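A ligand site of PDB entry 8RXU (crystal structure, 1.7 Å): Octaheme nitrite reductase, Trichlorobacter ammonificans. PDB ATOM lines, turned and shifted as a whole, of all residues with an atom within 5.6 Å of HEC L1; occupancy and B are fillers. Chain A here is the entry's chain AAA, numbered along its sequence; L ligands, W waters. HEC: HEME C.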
ATOM      1  N   ARG A   2      30.741 -17.589   4.386  1.00  0.00           N
ATOM      2  CA  ARG A   2      29.787 -18.713   4.635  1.00  0.00           C
ATOM      3  C   ARG A   2      29.392 -18.727   6.125  1.00  0.00           C
ATOM      4  O   ARG A   2      28.713 -19.673   6.569  1.00  0.00           O
ATOM      5  CB  ARG A   2      30.456 -20.039   4.273  1.00  0.00           C
ATOM      6  CG  ARG A   2      31.748 -20.299   5.047  1.00  0.00           C
ATOM      7  CD  ARG A   2      32.822 -21.106   4.315  1.00  0.00           C
ATOM      8  NE  ARG A   2      32.894 -20.750   2.907  1.00  0.00           N
ATOM      9  CZ  ARG A   2      33.527 -21.433   1.962  1.00  0.00           C
ATOM     10  NH1 ARG A   2      34.190 -22.542   2.249  1.00  0.00           N
ATOM     11  NH2 ARG A   2      33.489 -20.991   0.711  1.00  0.00           N
ATOM     12  N   THR A   4      27.582 -16.642   8.189  1.00  0.00           N
ATOM     13  CA  THR A   4      26.143 -16.412   8.484  1.00  0.00           C
ATOM     14  C   THR A   4      25.417 -17.761   8.534  1.00  0.00           C
ATOM     15  O   THR A   4      24.694 -18.040   9.530  1.00  0.00           O
ATOM     16  CB  THR A   4      25.474 -15.565   7.398  1.00  0.00           C
ATOM     17  OG1 THR A   4      26.420 -14.664   6.819  1.00  0.00           O
ATOM     18  CG2 THR A   4      24.280 -14.785   7.905  1.00  0.00           C
ATOM     19  N   CYS A   5      25.552 -18.520   7.442  1.00  0.00           N
ATOM     20  CA  CYS A   5      24.909 -19.836   7.230  1.00  0.00           C
ATOM     21  C   CYS A   5      25.194 -20.696   8.459  1.00  0.00           C
ATOM     22  O   CYS A   5      24.250 -21.237   9.121  1.00  0.00           O
ATOM     23  CB  CYS A   5      25.461 -20.505   5.968  1.00  0.00           C
ATOM     24  SG  CYS A   5      25.504 -19.516   4.477  1.00  0.00           S
ATOM     25  N   TYR A   6      26.490 -20.765   8.770  1.00  0.00           N
ATOM     26  CA  TYR A   6      27.074 -21.647   9.808  1.00  0.00           C
ATOM     27  C   TYR A   6      26.453 -21.329  11.167  1.00  0.00           C
ATOM     28  O   TYR A   6      26.238 -22.274  11.954  1.00  0.00           O
ATOM     29  CB  TYR A   6      28.588 -21.448   9.826  1.00  0.00           C
ATOM     30  CG  TYR A   6      29.344 -22.143   8.730  1.00  0.00           C
ATOM     31  CD1 TYR A   6      28.811 -23.218   8.019  1.00  0.00           C
ATOM     32  CD2 TYR A   6      30.651 -21.777   8.448  1.00  0.00           C
ATOM     33  CE1 TYR A   6      29.541 -23.878   7.042  1.00  0.00           C
ATOM     34  CE2 TYR A   6      31.397 -22.445   7.492  1.00  0.00           C
ATOM     35  CZ  TYR A   6      30.836 -23.479   6.772  1.00  0.00           C
ATOM     36  OH  TYR A   6      31.549 -24.099   5.804  1.00  0.00           O
ATOM     37  N   ALA A   7      26.109 -20.058  11.436  1.00  0.00           N
ATOM     38  CA  ALA A   7      25.586 -19.655  12.757  1.00  0.00           C
ATOM     39  C   ALA A   7      24.299 -20.429  13.100  1.00  0.00           C
ATOM     40  O   ALA A   7      24.077 -20.666  14.303  1.00  0.00           O
ATOM     41  CB  ALA A   7      25.384 -18.158  12.827  1.00  0.00           C
ATOM     42  N   CYS A   8      23.490 -20.832  12.102  1.00  0.00           N
ATOM     43  CA  CYS A   8      22.221 -21.589  12.362  1.00  0.00           C
ATOM     44  C   CYS A   8      22.319 -23.022  11.788  1.00  0.00           C
ATOM     45  O   CYS A   8      21.291 -23.742  11.857  1.00  0.00           O
ATOM     46  CB  CYS A   8      21.023 -20.830  11.781  1.00  0.00           C
ATOM     47  SG  CYS A   8      20.990 -19.043  12.038  1.00  0.00           S
ATOM     48  N   HIS A   9      23.471 -23.394  11.227  1.00  0.00           N
ATOM     49  CA  HIS A   9      23.723 -24.677  10.508  1.00  0.00           C
ATOM     50  C   HIS A   9      25.068 -25.289  10.912  1.00  0.00           C
ATOM     51  O   HIS A   9      26.012 -25.343  10.060  1.00  0.00           O
ATOM     52  CB  HIS A   9      23.737 -24.462   9.002  1.00  0.00           C
ATOM     53  CG  HIS A   9      22.433 -23.979   8.461  1.00  0.00           C
ATOM     54  ND1 HIS A   9      21.283 -24.699   8.629  1.00  0.00           N
ATOM     55  CD2 HIS A   9      22.104 -22.874   7.754  1.00  0.00           C
ATOM     56  CE1 HIS A   9      20.288 -24.068   8.009  1.00  0.00           C
ATOM     57  NE2 HIS A   9      20.761 -22.941   7.477  1.00  0.00           N
ATOM     58  N   CYS A  26      28.438 -22.295  -1.268  1.00  0.00           N
ATOM     59  CA  CYS A  26      27.087 -22.838  -0.968  1.00  0.00           C
ATOM     60  C   CYS A  26      26.220 -22.731  -2.213  1.00  0.00           C
ATOM     61  O   CYS A  26      25.390 -23.633  -2.435  1.00  0.00           O
ATOM     62  CB  CYS A  26      26.422 -22.046   0.156  1.00  0.00           C
ATOM     63  SG  CYS A  26      27.436 -21.962   1.608  1.00  0.00           S
ATOM     64  N   HIS A  30      22.915 -24.728  -3.801  1.00  0.00           N
ATOM     65  CA  HIS A  30      21.772 -24.091  -3.104  1.00  0.00           C
ATOM     66  C   HIS A  30      21.454 -22.786  -3.842  1.00  0.00           C
ATOM     67  O   HIS A  30      22.339 -21.938  -4.053  1.00  0.00           O
ATOM     68  CB  HIS A  30      22.045 -23.906  -1.606  1.00  0.00           C
ATOM     69  CG  HIS A  30      22.375 -25.150  -0.856  1.00  0.00           C
ATOM     70  ND1 HIS A  30      21.446 -26.134  -0.565  1.00  0.00           N
ATOM     71  CD2 HIS A  30      23.541 -25.584  -0.328  1.00  0.00           C
ATOM     72  CE1 HIS A  30      22.039 -27.108   0.120  1.00  0.00           C
ATOM     73  NE2 HIS A  30      23.311 -26.798   0.270  1.00  0.00           N
ATOM     74  N   THR A  33      19.289 -18.465  -1.618  1.00  0.00           N
ATOM     75  CA  THR A  33      20.027 -18.221  -0.348  1.00  0.00           C
ATOM     76  C   THR A  33      19.927 -16.726  -0.022  1.00  0.00           C
ATOM     77  O   THR A  33      19.555 -16.424   1.112  1.00  0.00           O
ATOM     78  CB  THR A  33      21.449 -18.783  -0.375  1.00  0.00           C
ATOM     79  OG1 THR A  33      22.151 -18.165  -1.456  1.00  0.00           O
ATOM     80  CG2 THR A  33      21.479 -20.293  -0.508  1.00  0.00           C
ATOM     81  N   HIS A  36      16.706 -16.602   1.257  1.00  0.00           N
ATOM     82  CA  HIS A  36      16.813 -17.234   2.599  1.00  0.00           C
ATOM     83  C   HIS A  36      17.390 -16.234   3.596  1.00  0.00           C
ATOM     84  O   HIS A  36      16.807 -16.101   4.649  1.00  0.00           O
ATOM     85  CB  HIS A  36      17.649 -18.537   2.517  1.00  0.00           C
ATOM     86  CG  HIS A  36      17.746 -19.377   3.753  1.00  0.00           C
ATOM     87  ND1 HIS A  36      16.642 -19.874   4.446  1.00  0.00           N
ATOM     88  CD2 HIS A  36      18.831 -19.920   4.371  1.00  0.00           C
ATOM     89  CE1 HIS A  36      17.044 -20.639   5.465  1.00  0.00           C
ATOM     90  NE2 HIS A  36      18.399 -20.673   5.451  1.00  0.00           N
ATOM     91  N   LEU A  37      18.468 -15.518   3.258  1.00  0.00           N
ATOM     92  CA  LEU A  37      19.144 -14.576   4.192  1.00  0.00           C
ATOM     93  C   LEU A  37      18.189 -13.425   4.559  1.00  0.00           C
ATOM     94  O   LEU A  37      17.892 -13.288   5.770  1.00  0.00           O
ATOM     95  CB  LEU A  37      20.445 -14.077   3.548  1.00  0.00           C
ATOM     96  CG  LEU A  37      21.493 -15.168   3.307  1.00  0.00           C
ATOM     97  CD1 LEU A  37      22.664 -14.632   2.481  1.00  0.00           C
ATOM     98  CD2 LEU A  37      21.976 -15.753   4.629  1.00  0.00           C
ATOM     99  N   PRO A  41      13.978 -17.558   7.721  1.00  0.00           N
ATOM    100  CA  PRO A  41      14.036 -19.010   7.539  1.00  0.00           C
ATOM    101  C   PRO A  41      12.787 -19.566   6.829  1.00  0.00           C
ATOM    102  O   PRO A  41      12.865 -20.676   6.351  1.00  0.00           O
ATOM    103  CB  PRO A  41      14.098 -19.525   8.979  1.00  0.00           C
ATOM    104  CG  PRO A  41      13.199 -18.554   9.725  1.00  0.00           C
ATOM    105  CD  PRO A  41      13.441 -17.212   9.051  1.00  0.00           C
ATOM    106  N   LYS A  44      12.998 -21.243   2.578  1.00  0.00           N
ATOM    107  CA  LYS A  44      13.982 -22.353   2.448  1.00  0.00           C
ATOM    108  C   LYS A  44      14.644 -22.270   1.081  1.00  0.00           C
ATOM    109  O   LYS A  44      13.932 -22.155   0.081  1.00  0.00           O
ATOM    110  CB  LYS A  44      13.232 -23.678   2.611  1.00  0.00           C
ATOM    111  CG  LYS A  44      12.699 -23.962   4.008  1.00  0.00           C
ATOM    112  CD  LYS A  44      11.520 -24.920   4.056  1.00  0.00           C
ATOM    113  CE  LYS A  44      10.203 -24.274   4.425  1.00  0.00           C
ATOM    114  NZ  LYS A  44       9.116 -24.682   3.498  1.00  0.00           N
ATOM    115  N   PRO A  45      15.991 -22.344   0.973  1.00  0.00           N
ATOM    116  CA  PRO A  45      16.670 -22.408  -0.330  1.00  0.00           C
ATOM    117  C   PRO A  45      16.238 -23.543  -1.276  1.00  0.00           C
ATOM    118  O   PRO A  45      15.623 -24.478  -0.824  1.00  0.00           O
ATOM    119  CB  PRO A  45      18.136 -22.677   0.055  1.00  0.00           C
ATOM    120  CG  PRO A  45      18.273 -22.083   1.426  1.00  0.00           C
ATOM    121  CD  PRO A  45      16.951 -22.403   2.094  1.00  0.00           C
ATOM    122  N   THR A  47      17.786 -26.577  -3.194  1.00  0.00           N
ATOM    123  CA  THR A  47      18.923 -27.518  -3.385  1.00  0.00           C
ATOM    124  C   THR A  47      18.434 -28.619  -4.329  1.00  0.00           C
ATOM    125  O   THR A  47      17.575 -29.410  -3.912  1.00  0.00           O
ATOM    126  CB  THR A  47      19.448 -28.044  -2.047  1.00  0.00           C
ATOM    127  OG1 THR A  47      20.393 -29.118  -2.228  1.00  0.00           O
ATOM    128  CG2 THR A  47      18.357 -28.526  -1.123  1.00  0.00           C
ATOM    129  N   LEU A 175      15.717 -34.415   1.401  1.00  0.00           N
ATOM    130  CA  LEU A 175      15.188 -33.262   2.181  1.00  0.00           C
ATOM    131  C   LEU A 175      13.659 -33.221   2.168  1.00  0.00           C
ATOM    132  O   LEU A 175      13.128 -32.123   2.374  1.00  0.00           O
ATOM    133  CB  LEU A 175      15.768 -31.944   1.661  1.00  0.00           C
ATOM    134  CG  LEU A 175      17.291 -31.894   1.552  1.00  0.00           C
ATOM    135  CD1 LEU A 175      17.770 -30.514   1.117  1.00  0.00           C
ATOM    136  CD2 LEU A 175      17.923 -32.311   2.872  1.00  0.00           C
ATOM    137  N   ARG A 251      18.106 -31.645  12.724  1.00  0.00           N
ATOM    138  CA  ARG A 251      16.803 -31.126  13.195  1.00  0.00           C
ATOM    139  C   ARG A 251      15.929 -32.212  13.828  1.00  0.00           C
ATOM    140  O   ARG A 251      14.716 -31.987  13.912  1.00  0.00           O
ATOM    141  CB  ARG A 251      16.072 -30.501  11.993  1.00  0.00           C
ATOM    142  CG  ARG A 251      16.912 -29.496  11.225  1.00  0.00           C
ATOM    143  CD  ARG A 251      16.232 -29.057   9.934  1.00  0.00           C
ATOM    144  NE  ARG A 251      16.604 -29.878   8.769  1.00  0.00           N
ATOM    145  CZ  ARG A 251      15.771 -30.580   7.992  1.00  0.00           C
ATOM    146  NH1 ARG A 251      14.477 -30.644   8.252  1.00  0.00           N
ATOM    147  NH2 ARG A 251      16.265 -31.280   6.972  1.00  0.00           N
HETATM  148 FE   HEC L   1      19.670 -21.844   6.331  1.00  0.00          FE
HETATM  149  CHA HEC L   1      17.120 -24.177   6.041  1.00  0.00           C
HETATM  150  CHB HEC L   1      21.227 -23.207   3.612  1.00  0.00           C
HETATM  151  CHC HEC L   1      21.796 -19.201   6.461  1.00  0.00           C
HETATM  152  CHD HEC L   1      18.477 -20.836   9.456  1.00  0.00           C
HETATM  153  NA  HEC L   1      19.245 -23.444   5.049  1.00  0.00           N
HETATM  154  C1A HEC L   1      18.167 -24.268   5.046  1.00  0.00           C
HETATM  155  C2A HEC L   1      18.115 -25.334   4.000  1.00  0.00           C
HETATM  156  C3A HEC L   1      19.346 -25.029   3.275  1.00  0.00           C
HETATM  157  C4A HEC L   1      19.974 -23.871   4.007  1.00  0.00           C
HETATM  158  CMA HEC L   1      19.865 -25.764   2.091  1.00  0.00           C
HETATM  159  CAA HEC L   1      17.060 -26.364   3.648  1.00  0.00           C
HETATM  160  CBA HEC L   1      16.867 -27.664   4.401  1.00  0.00           C
HETATM  161  CGA HEC L   1      15.553 -28.326   3.959  1.00  0.00           C
HETATM  162  O1A HEC L   1      14.870 -28.966   4.791  1.00  0.00           O
HETATM  163  O2A HEC L   1      15.167 -28.242   2.763  1.00  0.00           O
HETATM  164  NB  HEC L   1      21.261 -21.306   5.214  1.00  0.00           N
HETATM  165  C1B HEC L   1      21.750 -21.953   4.171  1.00  0.00           C
HETATM  166  C2B HEC L   1      22.853 -21.248   3.564  1.00  0.00           C
HETATM  167  C3B HEC L   1      23.013 -20.145   4.499  1.00  0.00           C
HETATM  168  C4B HEC L   1      21.950 -20.221   5.417  1.00  0.00           C
HETATM  169  CMB HEC L   1      23.662 -21.709   2.407  1.00  0.00           C
HETATM  170  CAB HEC L   1      23.915 -18.962   4.435  1.00  0.00           C
HETATM  171  CBB HEC L   1      23.515 -18.249   3.198  1.00  0.00           C
HETATM  172  NC  HEC L   1      20.022 -20.284   7.713  1.00  0.00           N
HETATM  173  C1C HEC L   1      20.920 -19.302   7.607  1.00  0.00           C
HETATM  174  C2C HEC L   1      21.015 -18.369   8.749  1.00  0.00           C
HETATM  175  C3C HEC L   1      19.982 -18.833   9.680  1.00  0.00           C
HETATM  176  C4C HEC L   1      19.497 -20.016   8.948  1.00  0.00           C
HETATM  177  CMC HEC L   1      21.949 -17.219   8.817  1.00  0.00           C
HETATM  178  CAC HEC L   1      19.672 -18.301  11.066  1.00  0.00           C
HETATM  179  CBC HEC L   1      18.352 -18.400  11.815  1.00  0.00           C
HETATM  180  ND  HEC L   1      18.138 -22.389   7.453  1.00  0.00           N
HETATM  181  C1D HEC L   1      17.822 -21.881   8.656  1.00  0.00           C
HETATM  182  C2D HEC L   1      16.613 -22.434   9.272  1.00  0.00           C
HETATM  183  C3D HEC L   1      16.193 -23.393   8.296  1.00  0.00           C
HETATM  184  C4D HEC L   1      17.205 -23.306   7.216  1.00  0.00           C
HETATM  185  CMD HEC L   1      16.026 -22.094  10.621  1.00  0.00           C
HETATM  186  CAD HEC L   1      15.042 -24.306   8.498  1.00  0.00           C
HETATM  187  CBD HEC L   1      13.640 -23.937   8.033  1.00  0.00           C
HETATM  188  CGD HEC L   1      12.863 -25.078   8.671  1.00  0.00           C
HETATM  189  O1D HEC L   1      11.742 -25.427   8.283  1.00  0.00           O
HETATM  190  O2D HEC L   1      13.404 -25.667   9.653  1.00  0.00           O
HETATM  191 FE   HEC L   2      24.410 -27.947   1.380  1.00  0.00          FE
HETATM  192  CHA HEC L   2      21.740 -29.873   2.590  1.00  0.00           C
HETATM  193  CHB HEC L   2      23.898 -25.670   3.850  1.00  0.00           C
HETATM  194  CHC HEC L   2      27.285 -26.196   0.500  1.00  0.00           C
HETATM  195  CHD HEC L   2      24.571 -29.903  -1.311  1.00  0.00           C
HETATM  196  NA  HEC L   2      23.086 -27.842   2.876  1.00  0.00           N
HETATM  197  C1A HEC L   2      22.075 -28.621   3.223  1.00  0.00           C
HETATM  198  C2A HEC L   2      21.362 -28.173   4.354  1.00  0.00           C
HETATM  199  C3A HEC L   2      21.979 -26.952   4.758  1.00  0.00           C
HETATM  200  C4A HEC L   2      23.026 -26.839   3.782  1.00  0.00           C
HETATM  201  CMA HEC L   2      21.599 -26.058   5.891  1.00  0.00           C
HETATM  202  CAA HEC L   2      20.241 -28.851   5.023  1.00  0.00           C
HETATM  203  CBA HEC L   2      20.873 -29.658   6.125  1.00  0.00           C
HETATM  204  CGA HEC L   2      19.775 -29.973   7.087  1.00  0.00           C
HETATM  205  O1A HEC L   2      19.299 -31.118   7.097  1.00  0.00           O
HETATM  206  O2A HEC L   2      19.382 -29.077   7.853  1.00  0.00           O
HETATM  207  NB  HEC L   2      25.416 -26.246   2.064  1.00  0.00           N
HETATM  208  C1B HEC L   2      25.074 -25.452   3.081  1.00  0.00           C
HETATM  209  C2B HEC L   2      25.933 -24.277   3.370  1.00  0.00           C
HETATM  210  C3B HEC L   2      26.957 -24.430   2.389  1.00  0.00           C
HETATM  211  C4B HEC L   2      26.536 -25.652   1.619  1.00  0.00           C
HETATM  212  CMB HEC L   2      25.770 -23.245   4.434  1.00  0.00           C
HETATM  213  CAB HEC L   2      28.102 -23.501   2.169  1.00  0.00           C
HETATM  214  CBB HEC L   2      29.097 -23.428   3.321  1.00  0.00           C
HETATM  215  NC  HEC L   2      25.729 -28.024  -0.185  1.00  0.00           N
HETATM  216  C1C HEC L   2      26.841 -27.304  -0.352  1.00  0.00           C
HETATM  217  C2C HEC L   2      27.534 -27.609  -1.556  1.00  0.00           C
HETATM  218  C3C HEC L   2      26.770 -28.744  -2.103  1.00  0.00           C
HETATM  219  C4C HEC L   2      25.650 -28.887  -1.192  1.00  0.00           C
HETATM  220  CMC HEC L   2      28.754 -26.954  -1.993  1.00  0.00           C
HETATM  221  CAC HEC L   2      27.006 -29.429  -3.391  1.00  0.00           C
HETATM  222  CBC HEC L   2      28.350 -30.054  -3.652  1.00  0.00           C
HETATM  223  ND  HEC L   2      23.318 -29.614   0.779  1.00  0.00           N
HETATM  224  C1D HEC L   2      23.531 -30.252  -0.351  1.00  0.00           C
HETATM  225  C2D HEC L   2      22.676 -31.399  -0.586  1.00  0.00           C
HETATM  226  C3D HEC L   2      21.820 -31.426   0.553  1.00  0.00           C
HETATM  227  C4D HEC L   2      22.333 -30.295   1.347  1.00  0.00           C
HETATM  228  CMD HEC L   2      22.709 -32.283  -1.793  1.00  0.00           C
HETATM  229  CAD HEC L   2      20.785 -32.462   0.834  1.00  0.00           C
HETATM  230  CBD HEC L   2      21.226 -33.239   2.100  1.00  0.00           C
HETATM  231  CGD HEC L   2      22.530 -34.075   2.115  1.00  0.00           C
HETATM  232  O1D HEC L   2      23.135 -34.234   3.240  1.00  0.00           O
HETATM  233  O2D HEC L   2      22.992 -34.637   1.086  1.00  0.00           O
HETATM  234  O   HOH W   1      15.089 -27.508   6.959  1.00  0.00           O
HETATM  235  O   HOH W   2      14.110 -21.234  12.830  1.00  0.00           O
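CAB of HEC L1 is covalently linked to SG of Cys 5 (1.7 Å). CAC of HEC L1 is covalently linked to SG of Cys 8 (1.8 Å). NE2 of His 9 is bound to FE of HEC L1 (1.9 Å). A ring nitrogen (NE2) of His 36 binds an iron atom (FE) of HEC L1, 1.9 Å away. NH2 of Arg 251 lies within salt-bridge range of O1A of HEC L1 (3.5 Å). NE2 of His 30 binds FE of HEC L2. NE of Arg 251 is in salt-bridge range of O2A of HEC L2 (3.0 Å). The side-chain sulfur of Cys 26 is covalently linked to a carbon (CAB) of HEC L2 (1.8 Å).
O of Thr 4 touches CMC of HEC L1, at 3.0 Å. Cys 26 touches HEC L1. His 30 touches HEC L1 (ND1 to CMA, 3.1 Å). Thr 33 touches HEC L1 (CG2 to CMB, 3.9 Å). Leu 37 touches HEC L1 (CD2 to CBB, 3.3 Å). Pro 41 touches HEC L1 (CB to CMD, 3.6 Å). Pro 45 touches HEC L1 (CG to C4A, 3.6 Å). CD1 of Leu 175 touches O2A of HEC L1, at 3.8 Å. Hydrophobic or aromatic side chains that line HEC L1: His 9, His 30, His 36, Leu 37, Pro 41, Pro 45 and Leu 175. Within 4 Å of HEC L1: Thr 4, Cys 5, Cys 8, His 9, Cys 26, His 30, Thr 33, His 36, Leu 37, Pro 41, Pro 45, Leu 175 and Arg 251. The nearest printed residue that does not touch HEC L1 is Lys 44 (4.1 Å).
Water W1 lies within hydrogen-bond range of O1A of HEC L1 (2.6 Å) and NE of Arg 251 (3.3 Å).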
